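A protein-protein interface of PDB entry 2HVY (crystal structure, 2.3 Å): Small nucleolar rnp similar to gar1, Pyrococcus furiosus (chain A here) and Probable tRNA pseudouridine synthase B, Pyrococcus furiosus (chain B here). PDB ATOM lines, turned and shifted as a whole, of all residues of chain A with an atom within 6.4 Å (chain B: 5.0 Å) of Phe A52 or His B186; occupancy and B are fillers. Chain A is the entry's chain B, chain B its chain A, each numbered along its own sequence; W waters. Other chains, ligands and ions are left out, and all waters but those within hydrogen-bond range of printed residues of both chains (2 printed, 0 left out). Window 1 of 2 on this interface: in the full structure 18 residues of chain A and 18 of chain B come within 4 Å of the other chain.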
ATOM      1  N   ILE A  24      11.157  16.731  18.020  1.00  0.00           N
ATOM      2  CA  ILE A  24      10.989  17.647  16.886  1.00  0.00           C
ATOM      3  C   ILE A  24       9.562  17.634  16.342  1.00  0.00           C
ATOM      4  O   ILE A  24       8.999  16.580  16.040  1.00  0.00           O
ATOM      5  CB  ILE A  24      12.049  17.424  15.765  1.00  0.00           C
ATOM      6  CG1 ILE A  24      13.365  18.114  16.133  1.00  0.00           C
ATOM      7  CG2 ILE A  24      11.591  18.023  14.432  1.00  0.00           C
ATOM      8  CD1 ILE A  24      14.275  17.308  16.991  1.00  0.00           C
ATOM      9  N   ASP A  50      14.549  25.617  20.342  1.00  0.00           N
ATOM     10  CA  ASP A  50      14.909  26.140  19.025  1.00  0.00           C
ATOM     11  C   ASP A  50      13.741  26.109  18.051  1.00  0.00           C
ATOM     12  O   ASP A  50      12.922  25.193  18.069  1.00  0.00           O
ATOM     13  CB  ASP A  50      16.103  25.381  18.430  1.00  0.00           C
ATOM     14  CG  ASP A  50      16.897  26.219  17.434  1.00  0.00           C
ATOM     15  OD1 ASP A  50      17.880  25.692  16.879  1.00  0.00           O
ATOM     16  OD2 ASP A  50      16.550  27.402  17.204  1.00  0.00           O
ATOM     17  N   VAL A  51      13.677  27.136  17.208  1.00  0.00           N
ATOM     18  CA  VAL A  51      12.699  27.221  16.128  1.00  0.00           C
ATOM     19  C   VAL A  51      13.475  27.517  14.851  1.00  0.00           C
ATOM     20  O   VAL A  51      14.241  28.480  14.786  1.00  0.00           O
ATOM     21  CB  VAL A  51      11.636  28.326  16.381  1.00  0.00           C
ATOM     22  CG1 VAL A  51      10.525  28.258  15.335  1.00  0.00           C
ATOM     23  CG2 VAL A  51      11.044  28.203  17.780  1.00  0.00           C
ATOM     24  N   PHE A  52      13.284  26.673  13.844  1.00  0.00           N
ATOM     25  CA  PHE A  52      14.075  26.735  12.619  1.00  0.00           C
ATOM     26  C   PHE A  52      13.279  26.249  11.406  1.00  0.00           C
ATOM     27  O   PHE A  52      12.128  25.838  11.538  1.00  0.00           O
ATOM     28  CB  PHE A  52      15.376  25.933  12.781  1.00  0.00           C
ATOM     29  CG  PHE A  52      15.169  24.496  13.202  1.00  0.00           C
ATOM     30  CD1 PHE A  52      14.955  24.169  14.539  1.00  0.00           C
ATOM     31  CD2 PHE A  52      15.200  23.471  12.261  1.00  0.00           C
ATOM     32  CE1 PHE A  52      14.763  22.844  14.930  1.00  0.00           C
ATOM     33  CE2 PHE A  52      15.021  22.141  12.645  1.00  0.00           C
ATOM     34  CZ  PHE A  52      14.799  21.827  13.982  1.00  0.00           C
ATOM     35  N   GLY A  53      13.900  26.309  10.230  1.00  0.00           N
ATOM     36  CA  GLY A  53      13.242  25.936   8.983  1.00  0.00           C
ATOM     37  C   GLY A  53      12.387  27.060   8.423  1.00  0.00           C
ATOM     38  O   GLY A  53      12.552  28.217   8.817  1.00  0.00           O
ATOM     39  N   PRO A  54      11.443  26.721   7.519  1.00  0.00           N
ATOM     40  CA  PRO A  54      10.633  27.716   6.802  1.00  0.00           C
ATOM     41  C   PRO A  54       9.795  28.556   7.757  1.00  0.00           C
ATOM     42  O   PRO A  54       9.207  28.021   8.694  1.00  0.00           O
ATOM     43  CB  PRO A  54       9.712  26.865   5.919  1.00  0.00           C
ATOM     44  CG  PRO A  54      10.300  25.507   5.904  1.00  0.00           C
ATOM     45  CD  PRO A  54      11.073  25.340   7.160  1.00  0.00           C
ATOM     46  N   VAL A  55       9.749  29.863   7.515  1.00  0.00           N
ATOM     47  CA  VAL A  55       8.991  30.784   8.365  1.00  0.00           C
ATOM     48  C   VAL A  55       7.500  30.408   8.454  1.00  0.00           C
ATOM     49  O   VAL A  55       6.895  30.511   9.521  1.00  0.00           O
ATOM     50  CB  VAL A  55       9.203  32.274   7.939  1.00  0.00           C
ATOM     51  CG1 VAL A  55       8.769  32.513   6.492  1.00  0.00           C
ATOM     52  CG2 VAL A  55       8.490  33.228   8.892  1.00  0.00           C
ATOM     53  N   MET A  57       6.177  27.308   7.822  1.00  0.00           N
ATOM     54  CA  MET A  57       6.012  25.950   8.347  1.00  0.00           C
ATOM     55  C   MET A  57       7.278  25.484   9.088  1.00  0.00           C
ATOM     56  O   MET A  57       7.998  24.606   8.605  1.00  0.00           O
ATOM     57  CB  MET A  57       5.654  24.985   7.211  1.00  0.00           C
ATOM     58  CG  MET A  57       4.908  23.736   7.653  1.00  0.00           C
ATOM     59  SD  MET A  57       3.134  24.006   7.860  1.00  0.00           S
ATOM     60  CE  MET A  57       2.732  22.661   8.977  1.00  0.00           C
ATOM     61  N   PRO A  58       7.557  26.076  10.266  1.00  0.00           N
ATOM     62  CA  PRO A  58       8.827  25.799  10.942  1.00  0.00           C
ATOM     63  C   PRO A  58       8.905  24.491  11.726  1.00  0.00           C
ATOM     64  O   PRO A  58       7.883  23.896  12.074  1.00  0.00           O
ATOM     65  CB  PRO A  58       8.982  26.991  11.893  1.00  0.00           C
ATOM     66  CG  PRO A  58       7.603  27.443  12.173  1.00  0.00           C
ATOM     67  CD  PRO A  58       6.732  27.044  11.014  1.00  0.00           C
ATOM     68  N   TYR A  59      10.136  24.055  11.975  1.00  0.00           N
ATOM     69  CA  TYR A  59      10.420  22.959  12.887  1.00  0.00           C
ATOM     70  C   TYR A  59      10.679  23.528  14.276  1.00  0.00           C
ATOM     71  O   TYR A  59      11.242  24.617  14.416  1.00  0.00           O
ATOM     72  CB  TYR A  59      11.646  22.175  12.424  1.00  0.00           C
ATOM     73  CG  TYR A  59      11.433  21.293  11.215  1.00  0.00           C
ATOM     74  CD1 TYR A  59      11.646  21.777   9.923  1.00  0.00           C
ATOM     75  CD2 TYR A  59      11.035  19.966  11.363  1.00  0.00           C
ATOM     76  CE1 TYR A  59      11.456  20.960   8.807  1.00  0.00           C
ATOM     77  CE2 TYR A  59      10.842  19.143  10.259  1.00  0.00           C
ATOM     78  CZ  TYR A  59      11.056  19.643   8.986  1.00  0.00           C
ATOM     79  OH  TYR A  59      10.864  18.821   7.898  1.00  0.00           O
ATOM     80  N   VAL A  60      10.261  22.791  15.300  1.00  0.00           N
ATOM     81  CA  VAL A  60      10.471  23.199  16.687  1.00  0.00           C
ATOM     82  C   VAL A  60      11.206  22.094  17.438  1.00  0.00           C
ATOM     83  O   VAL A  60      10.778  20.936  17.429  1.00  0.00           O
ATOM     84  CB  VAL A  60       9.129  23.539  17.402  1.00  0.00           C
ATOM     85  CG1 VAL A  60       9.380  24.039  18.808  1.00  0.00           C
ATOM     86  CG2 VAL A  60       8.348  24.590  16.622  1.00  0.00           C
ATOM     87  N   ALA A  61      12.323  22.454  18.068  1.00  0.00           N
ATOM     88  CA  ALA A  61      13.072  21.527  18.908  1.00  0.00           C
ATOM     89  C   ALA A  61      12.652  21.691  20.366  1.00  0.00           C
ATOM     90  O   ALA A  61      12.832  22.759  20.963  1.00  0.00           O
ATOM     91  CB  ALA A  61      14.576  21.739  18.745  1.00  0.00           C
ATOM     92  N   PHE B 132      14.006  23.623   3.140  1.00  0.00           N
ATOM     93  CA  PHE B 132      14.868  24.692   3.644  1.00  0.00           C
ATOM     94  C   PHE B 132      15.176  25.783   2.609  1.00  0.00           C
ATOM     95  O   PHE B 132      15.948  26.699   2.884  1.00  0.00           O
ATOM     96  CB  PHE B 132      16.148  24.117   4.262  1.00  0.00           C
ATOM     97  CG  PHE B 132      15.962  23.604   5.665  1.00  0.00           C
ATOM     98  CD1 PHE B 132      16.327  24.384   6.757  1.00  0.00           C
ATOM     99  CD2 PHE B 132      15.402  22.346   5.895  1.00  0.00           C
ATOM    100  CE1 PHE B 132      16.151  23.918   8.061  1.00  0.00           C
ATOM    101  CE2 PHE B 132      15.219  21.869   7.193  1.00  0.00           C
ATOM    102  CZ  PHE B 132      15.595  22.656   8.279  1.00  0.00           C
ATOM    103  N   ILE B 137      14.091  30.642   9.399  1.00  0.00           N
ATOM    104  CA  ILE B 137      14.376  31.269  10.688  1.00  0.00           C
ATOM    105  C   ILE B 137      15.810  30.974  11.132  1.00  0.00           C
ATOM    106  O   ILE B 137      16.204  29.810  11.244  1.00  0.00           O
ATOM    107  CB  ILE B 137      13.367  30.803  11.779  1.00  0.00           C
ATOM    108  CG1 ILE B 137      11.928  31.103  11.343  1.00  0.00           C
ATOM    109  CG2 ILE B 137      13.676  31.455  13.129  1.00  0.00           C
ATOM    110  CD1 ILE B 137      10.868  30.291  12.068  1.00  0.00           C
ATOM    111  N   SER B 182      25.172  26.244  10.646  1.00  0.00           N
ATOM    112  CA  SER B 182      23.907  26.272  11.370  1.00  0.00           C
ATOM    113  C   SER B 182      22.778  25.625  10.560  1.00  0.00           C
ATOM    114  O   SER B 182      21.988  24.848  11.105  1.00  0.00           O
ATOM    115  CB  SER B 182      23.544  27.711  11.746  1.00  0.00           C
ATOM    116  OG  SER B 182      22.349  27.748  12.501  1.00  0.00           O
ATOM    117  N   LEU B 183      22.714  25.953   9.269  1.00  0.00           N
ATOM    118  CA  LEU B 183      21.757  25.354   8.335  1.00  0.00           C
ATOM    119  C   LEU B 183      21.825  23.823   8.342  1.00  0.00           C
ATOM    120  O   LEU B 183      20.795  23.150   8.351  1.00  0.00           O
ATOM    121  CB  LEU B 183      21.985  25.895   6.913  1.00  0.00           C
ATOM    122  CG  LEU B 183      21.307  25.206   5.716  1.00  0.00           C
ATOM    123  CD1 LEU B 183      19.781  25.333   5.756  1.00  0.00           C
ATOM    124  CD2 LEU B 183      21.852  25.738   4.392  1.00  0.00           C
ATOM    125  N   ILE B 184      23.044  23.290   8.341  1.00  0.00           N
ATOM    126  CA  ILE B 184      23.263  21.849   8.337  1.00  0.00           C
ATOM    127  C   ILE B 184      22.841  21.210   9.665  1.00  0.00           C
ATOM    128  O   ILE B 184      22.188  20.160   9.676  1.00  0.00           O
ATOM    129  CB  ILE B 184      24.729  21.503   7.955  1.00  0.00           C
ATOM    130  CG1 ILE B 184      24.920  21.712   6.446  1.00  0.00           C
ATOM    131  CG2 ILE B 184      25.084  20.073   8.375  1.00  0.00           C
ATOM    132  CD1 ILE B 184      26.346  21.612   5.953  1.00  0.00           C
ATOM    133  N   HIS B 185      23.201  21.857  10.772  1.00  0.00           N
ATOM    134  CA  HIS B 185      22.787  21.418  12.103  1.00  0.00           C
ATOM    135  C   HIS B 185      21.266  21.320  12.206  1.00  0.00           C
ATOM    136  O   HIS B 185      20.741  20.367  12.777  1.00  0.00           O
ATOM    137  CB  HIS B 185      23.340  22.361  13.178  1.00  0.00           C
ATOM    138  CG  HIS B 185      22.848  22.057  14.559  1.00  0.00           C
ATOM    139  ND1 HIS B 185      23.338  21.011  15.312  1.00  0.00           N
ATOM    140  CD2 HIS B 185      21.905  22.658  15.322  1.00  0.00           C
ATOM    141  CE1 HIS B 185      22.718  20.983  16.478  1.00  0.00           C
ATOM    142  NE2 HIS B 185      21.845  21.972  16.510  1.00  0.00           N
ATOM    143  N   HIS B 186      20.568  22.300  11.635  1.00  0.00           N
ATOM    144  CA  HIS B 186      19.107  22.308  11.629  1.00  0.00           C
ATOM    145  C   HIS B 186      18.491  21.235  10.725  1.00  0.00           C
ATOM    146  O   HIS B 186      17.458  20.660  11.068  1.00  0.00           O
ATOM    147  CB  HIS B 186      18.575  23.699  11.278  1.00  0.00           C
ATOM    148  CG  HIS B 186      18.718  24.694  12.390  1.00  0.00           C
ATOM    149  ND1 HIS B 186      19.139  25.988  12.180  1.00  0.00           N
ATOM    150  CD2 HIS B 186      18.510  24.578  13.723  1.00  0.00           C
ATOM    151  CE1 HIS B 186      19.171  26.633  13.333  1.00  0.00           C
ATOM    152  NE2 HIS B 186      18.793  25.799  14.286  1.00  0.00           N
ATOM    153  N   ILE B 187      19.119  20.975   9.579  1.00  0.00           N
ATOM    154  CA  ILE B 187      18.687  19.894   8.686  1.00  0.00           C
ATOM    155  C   ILE B 187      18.800  18.540   9.404  1.00  0.00           C
ATOM    156  O   ILE B 187      17.896  17.705   9.315  1.00  0.00           O
ATOM    157  CB  ILE B 187      19.466  19.905   7.334  1.00  0.00           C
ATOM    158  CG1 ILE B 187      19.078  21.138   6.505  1.00  0.00           C
ATOM    159  CG2 ILE B 187      19.188  18.642   6.526  1.00  0.00           C
ATOM    160  CD1 ILE B 187      20.043  21.471   5.370  1.00  0.00           C
ATOM    161  N   GLY B 188      19.898  18.351  10.135  1.00  0.00           N
ATOM    162  CA  GLY B 188      20.103  17.157  10.958  1.00  0.00           C
ATOM    163  C   GLY B 188      19.037  16.945  12.021  1.00  0.00           C
ATOM    164  O   GLY B 188      18.661  15.809  12.303  1.00  0.00           O
ATOM    165  N   LEU B 189      18.545  18.038  12.604  1.00  0.00           N
ATOM    166  CA  LEU B 189      17.472  17.971  13.600  1.00  0.00           C
ATOM    167  C   LEU B 189      16.127  17.639  12.960  1.00  0.00           C
ATOM    168  O   LEU B 189      15.343  16.861  13.515  1.00  0.00           O
ATOM    169  CB  LEU B 189      17.372  19.279  14.391  1.00  0.00           C
ATOM    170  CG  LEU B 189      18.491  19.638  15.375  1.00  0.00           C
ATOM    171  CD1 LEU B 189      18.290  21.047  15.905  1.00  0.00           C
ATOM    172  CD2 LEU B 189      18.574  18.636  16.528  1.00  0.00           C
ATOM    173  N   ALA B 190      15.870  18.231  11.794  1.00  0.00           N
ATOM    174  CA  ALA B 190      14.658  17.958  11.018  1.00  0.00           C
ATOM    175  C   ALA B 190      14.628  16.520  10.491  1.00  0.00           C
ATOM    176  O   ALA B 190      13.557  15.946  10.298  1.00  0.00           O
ATOM    177  CB  ALA B 190      14.529  18.952   9.874  1.00  0.00           C
HETATM  178  O   HOH W   1      16.687  29.227  13.970  1.00  0.00           O
HETATM  179  O   HOH W   2      16.561  27.552   9.765  1.00  0.00           O
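The side-chain carboxylate (OD1) of Asp A50 lies within hydrogen-bond range of a ring nitrogen (NE2) of His B186 (2.8 Å).
The backbone NH of Ile B137 lies within hydrogen-bond range of the backbone carbonyl oxygen of Gly A53, 2.9 Å away.
The backbone NH (N) of Tyr A59 sits at hydrogen-bond distance from the backbone carbonyl oxygen (O) of Phe A52, at 2.7 Å.
The backbone carbonyl oxygen (O) of Ser B182 sits at hydrogen-bond distance from a ring nitrogen (ND1) of His B186 (3.3 Å).
The backbone carbonyl oxygen (O) of Asp A50 is in hydrogen-bond range of the backbone NH (N) of Ala A61 (2.8 Å).
Ile A24 touches Leu B189 (CG1 to O, 3.5 Å).
O of Val A51 touches CG2 of Ile B137, 3.5 Å away.
Ile B137 touches Phe A52.
Phe A52 touches His B186 (CE2 to O, 3.3 Å).
Phe A52 touches Leu B189.
CA of Gly A53 touches CE1 of Phe B132, at 3.7 Å.
Pro A58 touches Ile B137 (CB to CD1, 3.8 Å).
Ala B190 touches Tyr A59 (CB to CZ, 3.7 Å).
Printed residues of chain B within 4 Å of Ile A24: Leu B189.
Of the printed residues of chain B, Asp A50 touches His B186 (2.8 Å).
Of the printed residues of chain B, Phe A52 touches Ile B137, His B186 and Leu B189.
Printed residues of chain A within 4 Å of Phe B132: Gly A53 (3.7 Å).
His B186 touches just these residues of chain A: Asp A50 and Phe A52.
The nearest printed residue of chain B that does not touch Phe A52 is Phe B132 (4.1 Å).
The nearest residue of chain A that does not touch His B186 is Val A51 (5.3 Å).
The nearest printed residue of chain A that does not touch Phe B132 is Phe A52 (4.1 Å).
Hydrophobic or aromatic side chains of chain B within 4 Å of the printed part of chain A: Phe B132, Ile B137, His B186, Leu B189 and Ala B190.
Among the printed residues, no Asp or Glu carboxylate lies within 4 Å of a Lys or Arg side-chain nitrogen of the other chain.
Water W1 bridges the backbone carbonyl oxygen of Val A51 and the backbone carbonyl oxygen of Ile B137.
Water W2 lies within hydrogen-bond range of O of Ile B137 and N of Gly A53.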
